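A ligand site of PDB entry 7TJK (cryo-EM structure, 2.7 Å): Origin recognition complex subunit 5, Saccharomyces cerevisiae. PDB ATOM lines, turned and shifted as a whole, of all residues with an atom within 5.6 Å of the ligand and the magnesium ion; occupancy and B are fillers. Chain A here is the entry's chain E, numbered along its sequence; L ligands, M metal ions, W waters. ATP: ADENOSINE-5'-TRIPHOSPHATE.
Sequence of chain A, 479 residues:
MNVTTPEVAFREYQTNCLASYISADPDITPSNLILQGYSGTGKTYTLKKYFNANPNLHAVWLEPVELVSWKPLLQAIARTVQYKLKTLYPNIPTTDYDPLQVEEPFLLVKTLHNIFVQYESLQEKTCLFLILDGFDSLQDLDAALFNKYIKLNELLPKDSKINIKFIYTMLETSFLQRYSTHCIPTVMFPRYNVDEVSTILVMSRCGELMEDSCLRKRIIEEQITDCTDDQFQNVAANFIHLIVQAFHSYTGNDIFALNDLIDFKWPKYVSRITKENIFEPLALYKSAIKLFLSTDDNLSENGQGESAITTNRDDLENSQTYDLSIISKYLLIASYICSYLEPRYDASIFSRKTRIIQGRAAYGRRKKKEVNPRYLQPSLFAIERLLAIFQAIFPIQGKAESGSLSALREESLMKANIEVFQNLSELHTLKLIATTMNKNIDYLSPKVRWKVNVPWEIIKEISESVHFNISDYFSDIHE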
ATOM      1  N   VAL A   8     -17.958  -6.112 -24.937  1.00  0.00           N
ATOM      2  CA  VAL A   8     -18.821  -5.443 -25.896  1.00  0.00           C
ATOM      3  C   VAL A   8     -18.404  -3.985 -25.949  1.00  0.00           C
ATOM      4  O   VAL A   8     -18.143  -3.368 -24.918  1.00  0.00           O
ATOM      5  CB  VAL A   8     -20.309  -5.596 -25.510  1.00  0.00           C
ATOM      6  CG1 VAL A   8     -21.206  -5.165 -26.666  1.00  0.00           C
ATOM      7  CG2 VAL A   8     -20.601  -7.029 -25.120  1.00  0.00           C
ATOM      8  N   ALA A   9     -18.325  -3.441 -27.172  1.00  0.00           N
ATOM      9  CA  ALA A   9     -17.505  -2.255 -27.442  1.00  0.00           C
ATOM     10  C   ALA A   9     -18.059  -1.001 -26.790  1.00  0.00           C
ATOM     11  O   ALA A   9     -17.294  -0.086 -26.455  1.00  0.00           O
ATOM     12  CB  ALA A   9     -17.383  -2.055 -28.956  1.00  0.00           C
ATOM     13  N   PHE A  10     -19.369  -0.910 -26.620  1.00  0.00           N
ATOM     14  CA  PHE A  10     -19.986   0.260 -26.008  1.00  0.00           C
ATOM     15  C   PHE A  10     -21.038  -0.143 -24.992  1.00  0.00           C
ATOM     16  O   PHE A  10     -21.959   0.637 -24.698  1.00  0.00           O
ATOM     17  CB  PHE A  10     -20.572   1.193 -27.072  1.00  0.00           C
ATOM     18  CG  PHE A  10     -19.604   1.549 -28.168  1.00  0.00           C
ATOM     19  CD1 PHE A  10     -18.625   2.504 -27.969  1.00  0.00           C
ATOM     20  CD2 PHE A  10     -19.665   0.903 -29.390  1.00  0.00           C
ATOM     21  CE1 PHE A  10     -17.733   2.826 -28.963  1.00  0.00           C
ATOM     22  CE2 PHE A  10     -18.780   1.215 -30.397  1.00  0.00           C
ATOM     23  CZ  PHE A  10     -17.803   2.176 -30.185  1.00  0.00           C
ATOM     24  N   ARG A  11     -20.937  -1.353 -24.456  1.00  0.00           N
ATOM     25  CA  ARG A  11     -21.873  -1.886 -23.473  1.00  0.00           C
ATOM     26  C   ARG A  11     -21.116  -2.483 -22.287  1.00  0.00           C
ATOM     27  O   ARG A  11     -21.438  -3.566 -21.817  1.00  0.00           O
ATOM     28  CB  ARG A  11     -22.797  -2.930 -24.091  1.00  0.00           C
ATOM     29  CG  ARG A  11     -23.555  -2.505 -25.349  1.00  0.00           C
ATOM     30  CD  ARG A  11     -24.830  -1.728 -25.051  1.00  0.00           C
ATOM     31  NE  ARG A  11     -24.565  -0.307 -24.852  1.00  0.00           N
ATOM     32  CZ  ARG A  11     -25.494   0.644 -24.914  1.00  0.00           C
ATOM     33  NH1 ARG A  11     -26.750   0.363 -25.210  1.00  0.00           N
ATOM     34  NH2 ARG A  11     -25.136   1.900 -24.679  1.00  0.00           N
ATOM     35  N   GLY A  37     -34.524  -1.339 -23.083  1.00  0.00           N
ATOM     36  CA  GLY A  37     -33.902  -0.450 -24.046  1.00  0.00           C
ATOM     37  C   GLY A  37     -34.714  -0.446 -25.322  1.00  0.00           C
ATOM     38  O   GLY A  37     -35.456  -1.377 -25.613  1.00  0.00           O
ATOM     39  N   TYR A  38     -34.548   0.637 -26.076  1.00  0.00           N
ATOM     40  CA  TYR A  38     -35.282   0.761 -27.328  1.00  0.00           C
ATOM     41  C   TYR A  38     -34.618  -0.054 -28.428  1.00  0.00           C
ATOM     42  O   TYR A  38     -33.606  -0.734 -28.202  1.00  0.00           O
ATOM     43  CB  TYR A  38     -35.441   2.233 -27.695  1.00  0.00           C
ATOM     44  CG  TYR A  38     -36.526   2.904 -26.883  1.00  0.00           C
ATOM     45  CD1 TYR A  38     -37.844   2.916 -27.316  1.00  0.00           C
ATOM     46  CD2 TYR A  38     -36.227   3.496 -25.657  1.00  0.00           C
ATOM     47  CE1 TYR A  38     -38.833   3.516 -26.572  1.00  0.00           C
ATOM     48  CE2 TYR A  38     -37.214   4.094 -24.903  1.00  0.00           C
ATOM     49  CZ  TYR A  38     -38.510   4.102 -25.362  1.00  0.00           C
ATOM     50  OH  TYR A  38     -39.508   4.697 -24.617  1.00  0.00           O
ATOM     51  N   SER A  39     -35.195  -0.016 -29.616  1.00  0.00           N
ATOM     52  CA  SER A  39     -34.809  -0.919 -30.694  1.00  0.00           C
ATOM     53  C   SER A  39     -33.431  -0.565 -31.252  1.00  0.00           C
ATOM     54  O   SER A  39     -33.123   0.606 -31.488  1.00  0.00           O
ATOM     55  CB  SER A  39     -35.840  -0.896 -31.808  1.00  0.00           C
ATOM     56  OG  SER A  39     -35.440  -1.694 -32.906  1.00  0.00           O
ATOM     57  N   GLY A  40     -32.611  -1.584 -31.447  1.00  0.00           N
ATOM     58  CA  GLY A  40     -31.262  -1.390 -31.944  1.00  0.00           C
ATOM     59  C   GLY A  40     -30.285  -0.855 -30.925  1.00  0.00           C
ATOM     60  O   GLY A  40     -29.369  -0.111 -31.288  1.00  0.00           O
ATOM     61  N   THR A  41     -30.439  -1.209 -29.651  1.00  0.00           N
ATOM     62  CA  THR A  41     -29.543  -0.755 -28.605  1.00  0.00           C
ATOM     63  C   THR A  41     -28.618  -1.855 -28.097  1.00  0.00           C
ATOM     64  O   THR A  41     -27.952  -1.668 -27.081  1.00  0.00           O
ATOM     65  CB  THR A  41     -30.335  -0.172 -27.431  1.00  0.00           C
ATOM     66  OG1 THR A  41     -31.391  -1.062 -27.066  1.00  0.00           O
ATOM     67  CG2 THR A  41     -30.917   1.182 -27.818  1.00  0.00           C
ATOM     68  N   GLY A  42     -28.567  -2.994 -28.780  1.00  0.00           N
ATOM     69  CA  GLY A  42     -27.617  -4.035 -28.452  1.00  0.00           C
ATOM     70  C   GLY A  42     -27.983  -4.912 -27.274  1.00  0.00           C
ATOM     71  O   GLY A  42     -27.084  -5.505 -26.670  1.00  0.00           O
ATOM     72  N   LYS A  43     -29.261  -4.996 -26.911  1.00  0.00           N
ATOM     73  CA  LYS A  43     -29.692  -5.844 -25.808  1.00  0.00           C
ATOM     74  C   LYS A  43     -29.485  -7.318 -26.132  1.00  0.00           C
ATOM     75  O   LYS A  43     -28.845  -8.062 -25.357  1.00  0.00           O
ATOM     76  CB  LYS A  43     -31.165  -5.576 -25.490  1.00  0.00           C
ATOM     77  CG  LYS A  43     -31.477  -4.134 -25.144  1.00  0.00           C
ATOM     78  CD  LYS A  43     -32.932  -3.966 -24.780  1.00  0.00           C
ATOM     79  CE  LYS A  43     -33.828  -4.193 -25.992  1.00  0.00           C
ATOM     80  NZ  LYS A  43     -33.468  -3.347 -27.154  1.00  0.00           N
ATOM     81  N   THR A  44     -29.997  -7.755 -27.290  1.00  0.00           N
ATOM     82  CA  THR A  44     -29.857  -9.132 -27.723  1.00  0.00           C
ATOM     83  C   THR A  44     -28.405  -9.484 -27.985  1.00  0.00           C
ATOM     84  O   THR A  44     -27.946 -10.565 -27.623  1.00  0.00           O
ATOM     85  CB  THR A  44     -30.701  -9.380 -28.971  1.00  0.00           C
ATOM     86  OG1 THR A  44     -32.038  -8.903 -28.754  1.00  0.00           O
ATOM     87  CG2 THR A  44     -30.758 -10.864 -29.319  1.00  0.00           C
ATOM     88  N   TYR A  45     -27.656  -8.547 -28.573  1.00  0.00           N
ATOM     89  CA  TYR A  45     -26.244  -8.755 -28.875  1.00  0.00           C
ATOM     90  C   TYR A  45     -25.432  -8.967 -27.597  1.00  0.00           C
ATOM     91  O   TYR A  45     -24.624  -9.912 -27.510  1.00  0.00           O
ATOM     92  CB  TYR A  45     -25.705  -7.549 -29.661  1.00  0.00           C
ATOM     93  CG  TYR A  45     -24.306  -7.698 -30.197  1.00  0.00           C
ATOM     94  CD1 TYR A  45     -24.061  -8.394 -31.366  1.00  0.00           C
ATOM     95  CD2 TYR A  45     -23.221  -7.140 -29.518  1.00  0.00           C
ATOM     96  CE1 TYR A  45     -22.787  -8.531 -31.865  1.00  0.00           C
ATOM     97  CE2 TYR A  45     -21.945  -7.280 -30.008  1.00  0.00           C
ATOM     98  CZ  TYR A  45     -21.724  -7.973 -31.182  1.00  0.00           C
ATOM     99  OH  TYR A  45     -20.450  -8.106 -31.659  1.00  0.00           O
ATOM    100  N   THR A  46     -25.657  -8.129 -26.586  1.00  0.00           N
ATOM    101  CA  THR A  46     -24.927  -8.245 -25.331  1.00  0.00           C
ATOM    102  C   THR A  46     -25.304  -9.514 -24.582  1.00  0.00           C
ATOM    103  O   THR A  46     -24.448 -10.180 -23.987  1.00  0.00           O
ATOM    104  CB  THR A  46     -25.179  -7.006 -24.460  1.00  0.00           C
ATOM    105  OG1 THR A  46     -24.985  -5.823 -25.237  1.00  0.00           O
ATOM    106  CG2 THR A  46     -24.229  -6.965 -23.272  1.00  0.00           C
ATOM    107  N   ASP A 133     -37.277 -12.486 -24.693  1.00  0.00           N
ATOM    108  CA  ASP A 133     -36.712 -11.379 -25.456  1.00  0.00           C
ATOM    109  C   ASP A 133     -37.846 -10.666 -26.195  1.00  0.00           C
ATOM    110  O   ASP A 133     -38.236 -11.069 -27.285  1.00  0.00           O
ATOM    111  CB  ASP A 133     -35.652 -11.885 -26.422  1.00  0.00           C
ATOM    112  CG  ASP A 133     -34.603 -10.832 -26.736  1.00  0.00           C
ATOM    113  OD1 ASP A 133     -34.941  -9.634 -26.800  1.00  0.00           O
ATOM    114  OD2 ASP A 133     -33.425 -11.206 -26.929  1.00  0.00           O
ATOM    115  N   LEU A 171     -38.969  -2.864 -24.331  1.00  0.00           N
ATOM    116  CA  LEU A 171     -38.714  -1.761 -25.234  1.00  0.00           C
ATOM    117  C   LEU A 171     -39.115  -0.418 -24.643  1.00  0.00           C
ATOM    118  O   LEU A 171     -38.322   0.525 -24.631  1.00  0.00           O
ATOM    119  CB  LEU A 171     -39.429  -1.989 -26.574  1.00  0.00           C
ATOM    120  CG  LEU A 171     -38.734  -2.881 -27.605  1.00  0.00           C
ATOM    121  CD1 LEU A 171     -39.693  -3.304 -28.694  1.00  0.00           C
ATOM    122  CD2 LEU A 171     -37.529  -2.173 -28.190  1.00  0.00           C
ATOM    123  N   TYR A 192     -27.381   4.527 -28.750  1.00  0.00           N
ATOM    124  CA  TYR A 192     -26.023   4.855 -29.153  1.00  0.00           C
ATOM    125  C   TYR A 192     -25.970   6.267 -29.742  1.00  0.00           C
ATOM    126  O   TYR A 192     -26.950   6.759 -30.292  1.00  0.00           O
ATOM    127  CB  TYR A 192     -25.523   3.857 -30.202  1.00  0.00           C
ATOM    128  CG  TYR A 192     -25.358   2.434 -29.731  1.00  0.00           C
ATOM    129  CD1 TYR A 192     -24.354   2.088 -28.825  1.00  0.00           C
ATOM    130  CD2 TYR A 192     -26.187   1.427 -30.191  1.00  0.00           C
ATOM    131  CE1 TYR A 192     -24.192   0.782 -28.398  1.00  0.00           C
ATOM    132  CE2 TYR A 192     -26.045   0.114 -29.772  1.00  0.00           C
ATOM    133  CZ  TYR A 192     -25.039  -0.193 -28.878  1.00  0.00           C
ATOM    134  OH  TYR A 192     -24.893  -1.493 -28.457  1.00  0.00           O
ATOM    135  N   ILE A 200     -19.834   0.782 -34.820  1.00  0.00           N
ATOM    136  CA  ILE A 200     -20.545  -0.499 -34.877  1.00  0.00           C
ATOM    137  C   ILE A 200     -20.853  -0.875 -36.322  1.00  0.00           C
ATOM    138  O   ILE A 200     -20.664  -2.023 -36.720  1.00  0.00           O
ATOM    139  CB  ILE A 200     -21.816  -0.425 -34.007  1.00  0.00           C
ATOM    140  CG1 ILE A 200     -21.455  -0.568 -32.520  1.00  0.00           C
ATOM    141  CG2 ILE A 200     -22.841  -1.476 -34.398  1.00  0.00           C
ATOM    142  CD1 ILE A 200     -22.498  -0.009 -31.586  1.00  0.00           C
ATOM    143  N   MET A 203     -17.444  -1.965 -38.040  1.00  0.00           N
ATOM    144  CA  MET A 203     -16.928  -3.277 -37.662  1.00  0.00           C
ATOM    145  C   MET A 203     -17.949  -4.396 -37.840  1.00  0.00           C
ATOM    146  O   MET A 203     -17.577  -5.561 -37.691  1.00  0.00           O
ATOM    147  CB  MET A 203     -16.424  -3.285 -36.212  1.00  0.00           C
ATOM    148  CG  MET A 203     -17.490  -3.075 -35.159  1.00  0.00           C
ATOM    149  SD  MET A 203     -16.774  -3.051 -33.512  1.00  0.00           S
ATOM    150  CE  MET A 203     -18.236  -2.770 -32.523  1.00  0.00           C
ATOM    151  N   SER A 204     -19.195  -4.078 -38.161  1.00  0.00           N
ATOM    152  CA  SER A 204     -20.169  -5.109 -38.473  1.00  0.00           C
ATOM    153  C   SER A 204     -20.467  -5.235 -39.964  1.00  0.00           C
ATOM    154  O   SER A 204     -21.056  -6.246 -40.356  1.00  0.00           O
ATOM    155  CB  SER A 204     -21.491  -4.832 -37.732  1.00  0.00           C
ATOM    156  OG  SER A 204     -22.161  -3.711 -38.263  1.00  0.00           O
ATOM    157  N   ILE A 255     -29.673   1.752 -36.170  1.00  0.00           N
ATOM    158  CA  ILE A 255     -28.720   0.888 -36.856  1.00  0.00           C
ATOM    159  C   ILE A 255     -29.364   0.252 -38.079  1.00  0.00           C
ATOM    160  O   ILE A 255     -28.731   0.133 -39.141  1.00  0.00           O
ATOM    161  CB  ILE A 255     -28.177  -0.175 -35.878  1.00  0.00           C
ATOM    162  CG1 ILE A 255     -27.560   0.494 -34.653  1.00  0.00           C
ATOM    163  CG2 ILE A 255     -27.149  -1.077 -36.557  1.00  0.00           C
ATOM    164  CD1 ILE A 255     -26.950  -0.475 -33.655  1.00  0.00           C
ATOM    165  N   PHE A 256     -30.627  -0.156 -37.965  1.00  0.00           N
ATOM    166  CA  PHE A 256     -31.286  -0.921 -39.028  1.00  0.00           C
ATOM    167  C   PHE A 256     -31.547  -0.068 -40.268  1.00  0.00           C
ATOM    168  O   PHE A 256     -31.389  -0.553 -41.400  1.00  0.00           O
ATOM    169  CB  PHE A 256     -32.591  -1.526 -38.514  1.00  0.00           C
ATOM    170  CG  PHE A 256     -32.425  -2.365 -37.273  1.00  0.00           C
ATOM    171  CD1 PHE A 256     -31.675  -3.536 -37.314  1.00  0.00           C
ATOM    172  CD2 PHE A 256     -33.032  -2.001 -36.084  1.00  0.00           C
ATOM    173  CE1 PHE A 256     -31.526  -4.312 -36.180  1.00  0.00           C
ATOM    174  CE2 PHE A 256     -32.886  -2.769 -34.947  1.00  0.00           C
ATOM    175  CZ  PHE A 256     -32.133  -3.925 -34.995  1.00  0.00           C
HETATM  176  PG  ATP L   1     -34.590  -5.013 -30.785  1.00  0.00           P
HETATM  177  O1G ATP L   1     -35.255  -4.414 -29.590  1.00  0.00           O
HETATM  178  O2G ATP L   1     -35.076  -4.423 -32.097  1.00  0.00           O
HETATM  179  O3G ATP L   1     -34.700  -6.531 -30.859  1.00  0.00           O
HETATM  180  PB  ATP L   1     -31.772  -4.864 -29.807  1.00  0.00           P
HETATM  181  O1B ATP L   1     -31.628  -3.704 -28.915  1.00  0.00           O
HETATM  182  O2B ATP L   1     -31.892  -6.215 -29.116  1.00  0.00           O
HETATM  183  O3B ATP L   1     -33.017  -4.722 -30.778  1.00  0.00           O
HETATM  184  PA  ATP L   1     -29.562  -6.093 -31.337  1.00  0.00           P
HETATM  185  O1A ATP L   1     -30.227  -7.127 -32.150  1.00  0.00           O
HETATM  186  O2A ATP L   1     -28.853  -6.627 -30.096  1.00  0.00           O
HETATM  187  O3A ATP L   1     -30.576  -4.973 -30.849  1.00  0.00           O
HETATM  188  O5' ATP L   1     -28.509  -5.274 -32.191  1.00  0.00           O
HETATM  189  C5' ATP L   1     -28.713  -5.028 -33.599  1.00  0.00           C
HETATM  190  C4' ATP L   1     -27.509  -5.524 -34.360  1.00  0.00           C
HETATM  191  O4' ATP L   1     -26.516  -4.476 -34.424  1.00  0.00           O
HETATM  192  C3' ATP L   1     -26.795  -6.723 -33.741  1.00  0.00           C
HETATM  193  O3' ATP L   1     -27.358  -7.938 -34.209  1.00  0.00           O
HETATM  194  C2' ATP L   1     -25.357  -6.527 -34.223  1.00  0.00           C
HETATM  195  O2' ATP L   1     -25.169  -7.013 -35.549  1.00  0.00           O
HETATM  196  C1' ATP L   1     -25.228  -5.011 -34.185  1.00  0.00           C
HETATM  197  N9  ATP L   1     -24.730  -4.480 -32.917  1.00  0.00           N
HETATM  198  C8  ATP L   1     -25.466  -3.880 -31.928  1.00  0.00           C
HETATM  199  N7  ATP L   1     -24.750  -3.492 -30.895  1.00  0.00           N
HETATM  200  C5  ATP L   1     -23.464  -3.861 -31.233  1.00  0.00           C
HETATM  201  C6  ATP L   1     -22.232  -3.725 -30.569  1.00  0.00           C
HETATM  202  N6  ATP L   1     -22.088  -3.162 -29.361  1.00  0.00           N
HETATM  203  N1  ATP L   1     -21.127  -4.200 -31.180  1.00  0.00           N
HETATM  204  C2  ATP L   1     -21.247  -4.765 -32.382  1.00  0.00           C
HETATM  205  N3  ATP L   1     -22.354  -4.938 -33.110  1.00  0.00           N
HETATM  206  C4  ATP L   1     -23.433  -4.470 -32.475  1.00  0.00           C
HETATM  207 MG    MG M   1     -33.714  -8.141 -29.868  1.00  0.00          MG
HETATM  208  O   HOH W   1     -34.389  -7.498 -27.950  1.00  0.00           O
HETATM  209  O   HOH W   2     -35.178  -9.688 -30.232  1.00  0.00           O
HETATM  210  O   HOH W   3     -32.322  -8.229 -31.708  1.00  0.00           O
HETATM  211  O   HOH W   4     -36.068  -7.764 -32.944  1.00  0.00           O
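Water W1 lies within hydrogen-bond range of OD1 of Asp 133 and O2B of the ligand.
Residues that only touch the ligand: Val 8, Leu 171, Met 203, Ile 200, Tyr 38 and Phe 256.
Hydrophobic or aromatic side chains within 4 Å of the ligand: Val 8, Tyr 45, Leu 171, Tyr 192, Ile 200, Met 203 and Phe 256.
14 residues have an atom within 4 Å of the ligand: Val 8, Tyr 38, Ser 39, Gly 40, Thr 41, Gly 42, Lys 43, Thr 44, Tyr 45, Leu 171, Tyr 192, Ile 200, Met 203 and Phe 256.
The nearest printed residue that does not touch the ligand is Ile 255 (4.1 Å).
N of Thr 44 sits at hydrogen-bond distance from O2B of the ligand.
N of Lys 43 lies within hydrogen-bond range of O1B of the ligand, 3.4 Å away.
NZ of Lys 43 is in salt-bridge range of O1B of the ligand (2.6 Å).
An oxygen (O2A) of the ligand sits at hydrogen-bond distance from the backbone NH (N) of Tyr 45 (2.7 Å).
The backbone NH (N) of Thr 41 lies within hydrogen-bond range of an oxygen (O1B) of the ligand.
OG1 of Thr 41 lies within hydrogen-bond range of O1B of the ligand (3.2 Å).
The side-chain hydroxyl of Ser 39 sits at hydrogen-bond distance from an oxygen (O2G) of the ligand (2.9 Å).
The backbone NH (N) of Gly 42 is in hydrogen-bond range of an oxygen (O1B) of the ligand.
N7 of the ligand sits at hydrogen-bond distance from OH of Tyr 192, 3.2 Å away.
The backbone NH of Gly 40 lies within hydrogen-bond range of an oxygen (O3B) of the ligand (3.2 Å).
Merely in contact with the magnesium ion: Asp 133 (3.6 Å).
Along chain A the residues within 4 Å of the magnesium ion span positions 44 to 133.
The side-chain carboxylate (OD2) of Asp 133 lies close to the side-chain hydroxyl (OG1) of Thr 44 (3.2 Å).
OG1 of Thr 41 lies within hydrogen-bond range of NZ of Lys 43 (3.1 Å).
NZ of Lys 43 lies within hydrogen-bond range of O of Tyr 38 (2.8 Å).
NZ of Lys 43 is in hydrogen-bond range of O of Gly 37.
OH of Tyr 192 lies within hydrogen-bond range of O of Thr 41 (3.4 Å).
The backbone carbonyl oxygen of Thr 41 sits at hydrogen-bond distance from the guanidinium group of Arg 11 (3.0 Å).
The backbone carbonyl oxygen (O) of Gly 42 is in hydrogen-bond range of the side-chain hydroxyl (OG1) of Thr 46.
O of Ile 200 sits at hydrogen-bond distance from OG of Ser 204 (2.7 Å).
The magnesium ion is bound by an oxygen (O3G) of the ligand, water W1, the side-chain hydroxyl of Thr 44, water W2 and water W3.
The magnesium ion has five donor atoms within binding distance.
Slightly farther from the magnesium ion lies an oxygen (O2B) of the ligand (2.8 Å).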
